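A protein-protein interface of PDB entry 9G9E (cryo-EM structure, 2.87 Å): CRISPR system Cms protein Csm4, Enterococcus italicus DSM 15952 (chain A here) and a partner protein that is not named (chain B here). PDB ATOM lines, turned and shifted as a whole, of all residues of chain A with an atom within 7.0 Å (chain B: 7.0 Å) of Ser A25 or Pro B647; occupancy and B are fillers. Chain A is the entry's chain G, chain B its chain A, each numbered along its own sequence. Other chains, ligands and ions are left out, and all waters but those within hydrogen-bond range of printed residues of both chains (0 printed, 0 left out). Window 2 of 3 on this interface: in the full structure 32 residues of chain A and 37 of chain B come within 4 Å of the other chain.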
ATOM      1  N   HIS A  18      18.705 -17.269   9.711  1.00  0.00           N
ATOM      2  CA  HIS A  18      18.872 -16.912   8.306  1.00  0.00           C
ATOM      3  C   HIS A  18      20.358 -16.707   8.035  1.00  0.00           C
ATOM      4  O   HIS A  18      20.877 -15.598   8.179  1.00  0.00           O
ATOM      5  CB  HIS A  18      18.067 -15.666   7.953  1.00  0.00           C
ATOM      6  CG  HIS A  18      18.382 -15.116   6.597  1.00  0.00           C
ATOM      7  ND1 HIS A  18      18.233 -15.853   5.444  1.00  0.00           N
ATOM      8  CD2 HIS A  18      18.842 -13.903   6.213  1.00  0.00           C
ATOM      9  CE1 HIS A  18      18.591 -15.121   4.406  1.00  0.00           C
ATOM     10  NE2 HIS A  18      18.960 -13.932   4.844  1.00  0.00           N
ATOM     11  N   PHE A  19      21.039 -17.774   7.637  1.00  0.00           N
ATOM     12  CA  PHE A  19      22.435 -17.700   7.230  1.00  0.00           C
ATOM     13  C   PHE A  19      22.460 -17.570   5.713  1.00  0.00           C
ATOM     14  O   PHE A  19      22.093 -18.504   4.997  1.00  0.00           O
ATOM     15  CB  PHE A  19      23.213 -18.927   7.699  1.00  0.00           C
ATOM     16  CG  PHE A  19      23.295 -19.057   9.193  1.00  0.00           C
ATOM     17  CD1 PHE A  19      23.381 -17.934   9.996  1.00  0.00           C
ATOM     18  CD2 PHE A  19      23.297 -20.304   9.792  1.00  0.00           C
ATOM     19  CE1 PHE A  19      23.462 -18.052  11.369  1.00  0.00           C
ATOM     20  CE2 PHE A  19      23.379 -20.429  11.166  1.00  0.00           C
ATOM     21  CZ  PHE A  19      23.461 -19.300  11.954  1.00  0.00           C
ATOM     22  N   GLY A  20      22.872 -16.407   5.226  1.00  0.00           N
ATOM     23  CA  GLY A  20      22.862 -16.121   3.806  1.00  0.00           C
ATOM     24  C   GLY A  20      24.224 -16.307   3.166  1.00  0.00           C
ATOM     25  O   GLY A  20      25.257 -16.038   3.774  1.00  0.00           O
ATOM     26  N   LYS A  22      24.560 -15.426  -0.651  1.00  0.00           N
ATOM     27  CA  LYS A  22      24.549 -14.239  -1.495  1.00  0.00           C
ATOM     28  C   LYS A  22      23.210 -13.522  -1.535  1.00  0.00           C
ATOM     29  O   LYS A  22      23.173 -12.372  -1.980  1.00  0.00           O
ATOM     30  CB  LYS A  22      24.960 -14.603  -2.929  1.00  0.00           C
ATOM     31  CG  LYS A  22      26.363 -14.162  -3.304  1.00  0.00           C
ATOM     32  CD  LYS A  22      26.440 -13.756  -4.766  1.00  0.00           C
ATOM     33  CE  LYS A  22      27.751 -13.052  -5.076  1.00  0.00           C
ATOM     34  NZ  LYS A  22      28.317 -13.481  -6.384  1.00  0.00           N
ATOM     35  N   ARG A  23      22.120 -14.137  -1.080  1.00  0.00           N
ATOM     36  CA  ARG A  23      20.790 -13.560  -1.216  1.00  0.00           C
ATOM     37  C   ARG A  23      20.053 -13.650   0.111  1.00  0.00           C
ATOM     38  O   ARG A  23      20.446 -14.383   1.022  1.00  0.00           O
ATOM     39  CB  ARG A  23      19.983 -14.264  -2.313  1.00  0.00           C
ATOM     40  CG  ARG A  23      20.384 -13.879  -3.722  1.00  0.00           C
ATOM     41  CD  ARG A  23      20.172 -15.031  -4.687  1.00  0.00           C
ATOM     42  NE  ARG A  23      20.696 -14.722  -6.011  1.00  0.00           N
ATOM     43  CZ  ARG A  23      21.974 -14.813  -6.350  1.00  0.00           C
ATOM     44  NH1 ARG A  23      22.890 -15.230  -5.492  1.00  0.00           N
ATOM     45  NH2 ARG A  23      22.344 -14.477  -7.583  1.00  0.00           N
ATOM     46  N   LEU A  24      18.965 -12.886   0.208  1.00  0.00           N
ATOM     47  CA  LEU A  24      18.079 -12.965   1.362  1.00  0.00           C
ATOM     48  C   LEU A  24      17.207 -14.212   1.332  1.00  0.00           C
ATOM     49  O   LEU A  24      16.604 -14.559   2.353  1.00  0.00           O
ATOM     50  CB  LEU A  24      17.201 -11.711   1.432  1.00  0.00           C
ATOM     51  CG  LEU A  24      16.382 -11.447   2.698  1.00  0.00           C
ATOM     52  CD1 LEU A  24      17.285 -11.254   3.903  1.00  0.00           C
ATOM     53  CD2 LEU A  24      15.478 -10.241   2.505  1.00  0.00           C
ATOM     54  N   SER A  25      17.120 -14.890   0.188  1.00  0.00           N
ATOM     55  CA  SER A  25      16.370 -16.134   0.090  1.00  0.00           C
ATOM     56  C   SER A  25      17.210 -17.362   0.415  1.00  0.00           C
ATOM     57  O   SER A  25      16.651 -18.458   0.538  1.00  0.00           O
ATOM     58  CB  SER A  25      15.775 -16.277  -1.311  1.00  0.00           C
ATOM     59  OG  SER A  25      15.376 -15.017  -1.822  1.00  0.00           O
ATOM     60  N   ASP A  26      18.524 -17.211   0.556  1.00  0.00           N
ATOM     61  CA  ASP A  26      19.388 -18.351   0.835  1.00  0.00           C
ATOM     62  C   ASP A  26      19.238 -18.791   2.285  1.00  0.00           C
ATOM     63  O   ASP A  26      19.247 -17.963   3.201  1.00  0.00           O
ATOM     64  CB  ASP A  26      20.843 -17.996   0.535  1.00  0.00           C
ATOM     65  CG  ASP A  26      21.141 -17.965  -0.950  1.00  0.00           C
ATOM     66  OD1 ASP A  26      20.243 -18.311  -1.746  1.00  0.00           O
ATOM     67  OD2 ASP A  26      22.274 -17.594  -1.323  1.00  0.00           O
ATOM     68  N   SER A  27      19.101 -20.098   2.493  1.00  0.00           N
ATOM     69  CA  SER A  27      18.937 -20.685   3.823  1.00  0.00           C
ATOM     70  C   SER A  27      20.080 -21.667   4.061  1.00  0.00           C
ATOM     71  O   SER A  27      19.950 -22.871   3.832  1.00  0.00           O
ATOM     72  CB  SER A  27      17.556 -21.360   3.954  1.00  0.00           C
ATOM     73  OG  SER A  27      17.410 -22.432   3.039  1.00  0.00           O
ATOM     74  N   ASN A  28      21.207 -21.145   4.531  1.00  0.00           N
ATOM     75  CA  ASN A  28      22.336 -21.985   4.890  1.00  0.00           C
ATOM     76  C   ASN A  28      22.192 -22.469   6.328  1.00  0.00           C
ATOM     77  O   ASN A  28      21.641 -21.779   7.188  1.00  0.00           O
ATOM     78  CB  ASN A  28      23.653 -21.227   4.718  1.00  0.00           C
ATOM     79  CG  ASN A  28      24.851 -22.149   4.629  1.00  0.00           C
ATOM     80  OD1 ASN A  28      24.708 -23.350   4.401  1.00  0.00           O
ATOM     81  ND2 ASN A  28      26.042 -21.589   4.802  1.00  0.00           N
ATOM     82  N   SER A 130      13.557 -23.644   5.124  1.00  0.00           N
ATOM     83  CA  SER A 130      12.304 -23.166   4.561  1.00  0.00           C
ATOM     84  C   SER A 130      12.498 -21.732   4.083  1.00  0.00           C
ATOM     85  O   SER A 130      13.545 -21.117   4.305  1.00  0.00           O
ATOM     86  CB  SER A 130      11.169 -23.274   5.587  1.00  0.00           C
ATOM     87  OG  SER A 130       9.939 -22.795   5.071  1.00  0.00           O
ATOM     88  N   LEU A 131      11.473 -21.195   3.424  1.00  0.00           N
ATOM     89  CA  LEU A 131      11.511 -19.843   2.864  1.00  0.00           C
ATOM     90  C   LEU A 131      10.231 -19.123   3.275  1.00  0.00           C
ATOM     91  O   LEU A 131       9.153 -19.415   2.749  1.00  0.00           O
ATOM     92  CB  LEU A 131      11.663 -19.884   1.350  1.00  0.00           C
ATOM     93  CG  LEU A 131      11.915 -18.554   0.643  1.00  0.00           C
ATOM     94  CD1 LEU A 131      13.197 -18.612  -0.160  1.00  0.00           C
ATOM     95  CD2 LEU A 131      10.736 -18.220  -0.251  1.00  0.00           C
ATOM     96  N   TYR A 149       8.717  -9.961  -0.179  1.00  0.00           N
ATOM     97  CA  TYR A 149      10.084 -10.448  -0.291  1.00  0.00           C
ATOM     98  C   TYR A 149      10.165 -11.799   0.408  1.00  0.00           C
ATOM     99  O   TYR A 149       9.185 -12.283   0.979  1.00  0.00           O
ATOM    100  CB  TYR A 149      11.087  -9.438   0.280  1.00  0.00           C
ATOM    101  CG  TYR A 149      10.939  -9.158   1.759  1.00  0.00           C
ATOM    102  CD1 TYR A 149       9.944  -8.313   2.230  1.00  0.00           C
ATOM    103  CD2 TYR A 149      11.807  -9.726   2.681  1.00  0.00           C
ATOM    104  CE1 TYR A 149       9.811  -8.051   3.579  1.00  0.00           C
ATOM    105  CE2 TYR A 149      11.681  -9.469   4.032  1.00  0.00           C
ATOM    106  CZ  TYR A 149      10.681  -8.630   4.474  1.00  0.00           C
ATOM    107  OH  TYR A 149      10.551  -8.372   5.818  1.00  0.00           O
ATOM    108  N   SER A 150      11.341 -12.418   0.349  1.00  0.00           N
ATOM    109  CA  SER A 150      11.537 -13.758   0.880  1.00  0.00           C
ATOM    110  C   SER A 150      12.753 -13.791   1.793  1.00  0.00           C
ATOM    111  O   SER A 150      13.778 -13.170   1.497  1.00  0.00           O
ATOM    112  CB  SER A 150      11.712 -14.778  -0.250  1.00  0.00           C
ATOM    113  OG  SER A 150      10.545 -14.862  -1.047  1.00  0.00           O
ATOM    114  N   VAL A 151      12.631 -14.517   2.901  1.00  0.00           N
ATOM    115  CA  VAL A 151      13.734 -14.750   3.826  1.00  0.00           C
ATOM    116  C   VAL A 151      13.900 -16.256   3.976  1.00  0.00           C
ATOM    117  O   VAL A 151      12.963 -16.949   4.388  1.00  0.00           O
ATOM    118  CB  VAL A 151      13.491 -14.087   5.192  1.00  0.00           C
ATOM    119  CG1 VAL A 151      14.695 -14.283   6.098  1.00  0.00           C
ATOM    120  CG2 VAL A 151      13.190 -12.609   5.018  1.00  0.00           C
ATOM    121  N   GLY A 152      15.081 -16.760   3.636  1.00  0.00           N
ATOM    122  CA  GLY A 152      15.335 -18.182   3.743  1.00  0.00           C
ATOM    123  C   GLY A 152      15.885 -18.578   5.096  1.00  0.00           C
ATOM    124  O   GLY A 152      17.045 -18.299   5.405  1.00  0.00           O
ATOM    125  N   ASN A 153      15.077 -19.254   5.904  1.00  0.00           N
ATOM    126  CA  ASN A 153      15.459 -19.602   7.262  1.00  0.00           C
ATOM    127  C   ASN A 153      15.737 -21.096   7.364  1.00  0.00           C
ATOM    128  O   ASN A 153      15.419 -21.879   6.468  1.00  0.00           O
ATOM    129  CB  ASN A 153      14.371 -19.193   8.265  1.00  0.00           C
ATOM    130  CG  ASN A 153      12.973 -19.452   7.749  1.00  0.00           C
ATOM    131  OD1 ASN A 153      12.331 -18.564   7.189  1.00  0.00           O
ATOM    132  ND2 ASN A 153      12.489 -20.673   7.939  1.00  0.00           N
ATOM    133  N   TYR B 284      22.031 -20.705 -12.574  1.00  0.00           N
ATOM    134  CA  TYR B 284      20.830 -20.646 -11.750  1.00  0.00           C
ATOM    135  C   TYR B 284      20.910 -19.682 -10.578  1.00  0.00           C
ATOM    136  O   TYR B 284      19.866 -19.222 -10.114  1.00  0.00           O
ATOM    137  CB  TYR B 284      20.486 -22.045 -11.228  1.00  0.00           C
ATOM    138  CG  TYR B 284      20.255 -23.040 -12.341  1.00  0.00           C
ATOM    139  CD1 TYR B 284      19.140 -22.944 -13.163  1.00  0.00           C
ATOM    140  CD2 TYR B 284      21.159 -24.065 -12.582  1.00  0.00           C
ATOM    141  CE1 TYR B 284      18.928 -23.844 -14.186  1.00  0.00           C
ATOM    142  CE2 TYR B 284      20.955 -24.971 -13.604  1.00  0.00           C
ATOM    143  CZ  TYR B 284      19.838 -24.857 -14.403  1.00  0.00           C
ATOM    144  OH  TYR B 284      19.630 -25.756 -15.422  1.00  0.00           O
ATOM    145  N   ILE B 286      21.021 -16.562  -9.978  1.00  0.00           N
ATOM    146  CA  ILE B 286      20.798 -15.236 -10.535  1.00  0.00           C
ATOM    147  C   ILE B 286      19.555 -14.637  -9.890  1.00  0.00           C
ATOM    148  O   ILE B 286      18.679 -15.347  -9.391  1.00  0.00           O
ATOM    149  CB  ILE B 286      20.655 -15.260 -12.073  1.00  0.00           C
ATOM    150  CG1 ILE B 286      19.534 -16.211 -12.494  1.00  0.00           C
ATOM    151  CG2 ILE B 286      21.970 -15.649 -12.729  1.00  0.00           C
ATOM    152  CD1 ILE B 286      19.312 -16.261 -13.989  1.00  0.00           C
ATOM    153  N   GLY B 288      16.743 -10.913  -9.864  1.00  0.00           N
ATOM    154  CA  GLY B 288      15.983 -10.035 -10.724  1.00  0.00           C
ATOM    155  C   GLY B 288      14.698 -10.679 -11.219  1.00  0.00           C
ATOM    156  O   GLY B 288      14.509 -11.897 -11.165  1.00  0.00           O
ATOM    157  N   TYR B 642       6.262 -24.087  -7.898  1.00  0.00           N
ATOM    158  CA  TYR B 642       6.590 -22.806  -7.298  1.00  0.00           C
ATOM    159  C   TYR B 642       5.714 -21.710  -7.882  1.00  0.00           C
ATOM    160  O   TYR B 642       5.267 -21.810  -9.026  1.00  0.00           O
ATOM    161  CB  TYR B 642       8.067 -22.458  -7.537  1.00  0.00           C
ATOM    162  CG  TYR B 642       9.015 -23.586  -7.212  1.00  0.00           C
ATOM    163  CD1 TYR B 642       9.426 -23.821  -5.909  1.00  0.00           C
ATOM    164  CD2 TYR B 642       9.499 -24.419  -8.212  1.00  0.00           C
ATOM    165  CE1 TYR B 642      10.290 -24.854  -5.611  1.00  0.00           C
ATOM    166  CE2 TYR B 642      10.364 -25.454  -7.922  1.00  0.00           C
ATOM    167  CZ  TYR B 642      10.757 -25.666  -6.620  1.00  0.00           C
ATOM    168  OH  TYR B 642      11.620 -26.695  -6.326  1.00  0.00           O
ATOM    169  N   PRO B 643       5.448 -20.653  -7.122  1.00  0.00           N
ATOM    170  CA  PRO B 643       4.753 -19.499  -7.697  1.00  0.00           C
ATOM    171  C   PRO B 643       5.646 -18.762  -8.682  1.00  0.00           C
ATOM    172  O   PRO B 643       6.868 -18.910  -8.688  1.00  0.00           O
ATOM    173  CB  PRO B 643       4.430 -18.623  -6.480  1.00  0.00           C
ATOM    174  CG  PRO B 643       4.648 -19.502  -5.283  1.00  0.00           C
ATOM    175  CD  PRO B 643       5.688 -20.494  -5.679  1.00  0.00           C
ATOM    176  N   VAL B 644       5.011 -17.973  -9.548  1.00  0.00           N
ATOM    177  CA  VAL B 644       5.773 -17.037 -10.360  1.00  0.00           C
ATOM    178  C   VAL B 644       6.363 -15.970  -9.444  1.00  0.00           C
ATOM    179  O   VAL B 644       5.828 -15.681  -8.363  1.00  0.00           O
ATOM    180  CB  VAL B 644       4.901 -16.418 -11.468  1.00  0.00           C
ATOM    181  CG1 VAL B 644       4.080 -15.255 -10.933  1.00  0.00           C
ATOM    182  CG2 VAL B 644       5.766 -15.980 -12.642  1.00  0.00           C
ATOM    183  N   LYS B 645       7.501 -15.411  -9.855  1.00  0.00           N
ATOM    184  CA  LYS B 645       8.334 -14.468  -9.107  1.00  0.00           C
ATOM    185  C   LYS B 645       9.081 -15.170  -7.976  1.00  0.00           C
ATOM    186  O   LYS B 645       9.799 -14.500  -7.223  1.00  0.00           O
ATOM    187  CB  LYS B 645       7.546 -13.280  -8.530  1.00  0.00           C
ATOM    188  CG  LYS B 645       6.915 -12.384  -9.580  1.00  0.00           C
ATOM    189  CD  LYS B 645       5.805 -11.535  -8.984  1.00  0.00           C
ATOM    190  CE  LYS B 645       6.298 -10.736  -7.789  1.00  0.00           C
ATOM    191  NZ  LYS B 645       5.200  -9.952  -7.160  1.00  0.00           N
ATOM    192  N   TYR B 646       8.932 -16.482  -7.826  1.00  0.00           N
ATOM    193  CA  TYR B 646       9.746 -17.226  -6.879  1.00  0.00           C
ATOM    194  C   TYR B 646      11.212 -17.146  -7.300  1.00  0.00           C
ATOM    195  O   TYR B 646      11.509 -17.124  -8.500  1.00  0.00           O
ATOM    196  CB  TYR B 646       9.288 -18.685  -6.826  1.00  0.00           C
ATOM    197  CG  TYR B 646       9.707 -19.459  -5.597  1.00  0.00           C
ATOM    198  CD1 TYR B 646       8.981 -19.373  -4.418  1.00  0.00           C
ATOM    199  CD2 TYR B 646      10.813 -20.296  -5.626  1.00  0.00           C
ATOM    200  CE1 TYR B 646       9.355 -20.087  -3.297  1.00  0.00           C
ATOM    201  CE2 TYR B 646      11.194 -21.013  -4.510  1.00  0.00           C
ATOM    202  CZ  TYR B 646      10.463 -20.905  -3.349  1.00  0.00           C
ATOM    203  OH  TYR B 646      10.839 -21.618  -2.236  1.00  0.00           O
ATOM    204  N   PRO B 647      12.146 -17.078  -6.352  1.00  0.00           N
ATOM    205  CA  PRO B 647      13.565 -17.004  -6.727  1.00  0.00           C
ATOM    206  C   PRO B 647      13.972 -18.203  -7.572  1.00  0.00           C
ATOM    207  O   PRO B 647      13.735 -19.354  -7.202  1.00  0.00           O
ATOM    208  CB  PRO B 647      14.289 -16.987  -5.376  1.00  0.00           C
ATOM    209  CG  PRO B 647      13.273 -16.503  -4.402  1.00  0.00           C
ATOM    210  CD  PRO B 647      11.953 -17.006  -4.895  1.00  0.00           C
ATOM    211  N   ILE B 648      14.588 -17.918  -8.721  1.00  0.00           N
ATOM    212  CA  ILE B 648      14.979 -18.984  -9.636  1.00  0.00           C
ATOM    213  C   ILE B 648      16.080 -19.836  -9.014  1.00  0.00           C
ATOM    214  O   ILE B 648      16.107 -21.061  -9.194  1.00  0.00           O
ATOM    215  CB  ILE B 648      15.406 -18.380 -10.990  1.00  0.00           C
ATOM    216  CG1 ILE B 648      16.071 -19.425 -11.892  1.00  0.00           C
ATOM    217  CG2 ILE B 648      16.326 -17.189 -10.775  1.00  0.00           C
ATOM    218  CD1 ILE B 648      15.232 -20.673 -12.124  1.00  0.00           C
ATOM    219  N   SER B 649      16.995 -19.215  -8.267  1.00  0.00           N
ATOM    220  CA  SER B 649      18.019 -19.983  -7.566  1.00  0.00           C
ATOM    221  C   SER B 649      17.391 -20.936  -6.558  1.00  0.00           C
ATOM    222  O   SER B 649      17.810 -22.094  -6.442  1.00  0.00           O
ATOM    223  CB  SER B 649      19.003 -19.039  -6.876  1.00  0.00           C
ATOM    224  OG  SER B 649      18.320 -18.019  -6.171  1.00  0.00           O
ATOM    225  N   LYS B 650      16.379 -20.467  -5.823  1.00  0.00           N
ATOM    226  CA  LYS B 650      15.663 -21.348  -4.905  1.00  0.00           C
ATOM    227  C   LYS B 650      14.942 -22.459  -5.656  1.00  0.00           C
ATOM    228  O   LYS B 650      14.931 -23.608  -5.202  1.00  0.00           O
ATOM    229  CB  LYS B 650      14.678 -20.543  -4.058  1.00  0.00           C
ATOM    230  CG  LYS B 650      15.340 -19.624  -3.049  1.00  0.00           C
ATOM    231  CD  LYS B 650      16.242 -20.410  -2.111  1.00  0.00           C
ATOM    232  CE  LYS B 650      15.431 -21.303  -1.185  1.00  0.00           C
ATOM    233  NZ  LYS B 650      16.263 -21.885  -0.096  1.00  0.00           N
ATOM    234  N   MET B 651      14.332 -22.136  -6.799  1.00  0.00           N
ATOM    235  CA  MET B 651      13.698 -23.161  -7.621  1.00  0.00           C
ATOM    236  C   MET B 651      14.687 -24.263  -7.972  1.00  0.00           C
ATOM    237  O   MET B 651      14.427 -25.450  -7.742  1.00  0.00           O
ATOM    238  CB  MET B 651      13.141 -22.537  -8.903  1.00  0.00           C
ATOM    239  CG  MET B 651      11.956 -21.608  -8.724  1.00  0.00           C
ATOM    240  SD  MET B 651      11.504 -20.845 -10.296  1.00  0.00           S
ATOM    241  CE  MET B 651       9.798 -20.393 -10.001  1.00  0.00           C
ATOM    242  N   ALA B 652      15.842 -23.876  -8.517  1.00  0.00           N
ATOM    243  CA  ALA B 652      16.833 -24.854  -8.950  1.00  0.00           C
ATOM    244  C   ALA B 652      17.365 -25.660  -7.772  1.00  0.00           C
ATOM    245  O   ALA B 652      17.500 -26.885  -7.857  1.00  0.00           O
ATOM    246  CB  ALA B 652      17.972 -24.153  -9.686  1.00  0.00           C
ATOM    247  N   SER B 653      17.668 -24.988  -6.658  1.00  0.00           N
ATOM    248  CA  SER B 653      18.228 -25.688  -5.506  1.00  0.00           C
ATOM    249  C   SER B 653      17.229 -26.675  -4.914  1.00  0.00           C
ATOM    250  O   SER B 653      17.596 -27.805  -4.572  1.00  0.00           O
ATOM    251  CB  SER B 653      18.682 -24.682  -4.449  1.00  0.00           C
ATOM    252  OG  SER B 653      17.629 -23.806  -4.092  1.00  0.00           O
ATOM    253  N   GLU B 654      15.960 -26.280  -4.800  1.00  0.00           N
ATOM    254  CA  GLU B 654      14.971 -27.170  -4.203  1.00  0.00           C
ATOM    255  C   GLU B 654      14.633 -28.328  -5.135  1.00  0.00           C
ATOM    256  O   GLU B 654      14.420 -29.457  -4.676  1.00  0.00           O
ATOM    257  CB  GLU B 654      13.719 -26.381  -3.822  1.00  0.00           C
ATOM    258  CG  GLU B 654      13.961 -25.391  -2.690  1.00  0.00           C
ATOM    259  CD  GLU B 654      12.719 -24.612  -2.306  1.00  0.00           C
ATOM    260  OE1 GLU B 654      11.649 -24.867  -2.893  1.00  0.00           O
ATOM    261  OE2 GLU B 654      12.815 -23.739  -1.418  1.00  0.00           O
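NZ of Lys B650 sits at hydrogen-bond distance from OG of Ser A27, 3.4 Å away. The guanidinium group of Arg A23 lies close to the backbone NH of Ile B286, 3.4 Å away.
The backbone NH of Ser B649 sits close to the backbone carbonyl oxygen of Tyr B284, at 3.4 Å. OE2 of Glu B654 lies within hydrogen-bond range of OH of Tyr B646. The backbone carbonyl oxygen (O) of Ser B649 sits at hydrogen-bond distance from the side-chain hydroxyl (OG) of Ser B653, at 2.9 Å. O of Lys B650 sits at hydrogen-bond distance from OG of Ser B653 (2.9 Å). The backbone NH of Arg A23 lies within hydrogen-bond range of the side-chain carboxylate of Asp A26.
CD of Arg A23 touches OG of Ser B649, 3.8 Å away. Pro B647 touches Ser A25. O of Ser A25 touches CD of Lys B650, 3.3 Å away. Leu A131 touches Tyr B646 (CD2 to CE1, 3.8 Å). Leu A131 touches Lys B650.
Ser A25 touches just these residues of chain B: Pro B647 and Lys B650. Pro B647 touches just one residue of chain A: Ser A25. Of the printed residues of chain B, Leu A131 touches Tyr B646 and Lys B650. Of the printed residues of chain B, Arg A23 touches Ile B286 (3.4 Å) and Ser B649 (3.8 Å). Of the printed residues of chain A, Lys B650 touches Ser A25 (3.3 Å), Ser A27 (3.4 Å) and Leu A131 (3.6 Å). Of the printed residues of chain A, Ile B286 touches Arg A23 (3.4 Å). Of the printed residues of chain B, Ser A27 touches Lys B650. His A18 touches none of the printed residues of chain B. The nearest residue of chain A that does not touch Pro B647 is Ser A150 (4.6 Å). The nearest printed residue of chain B that does not touch Ser A27 is Glu B654 (6.5 Å).
Of the 16 printed residues of chain B, 5 touch a printed residue of chain A. Printed residues of chain B that touch a printed residue of chain A: Ile B286, Tyr B646, Pro B647, Ser B649 and Lys B650. Of the 17 printed residues of chain A, 4 touch a printed residue of chain B. Among the printed residues, 7 pairs touch across the chains.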
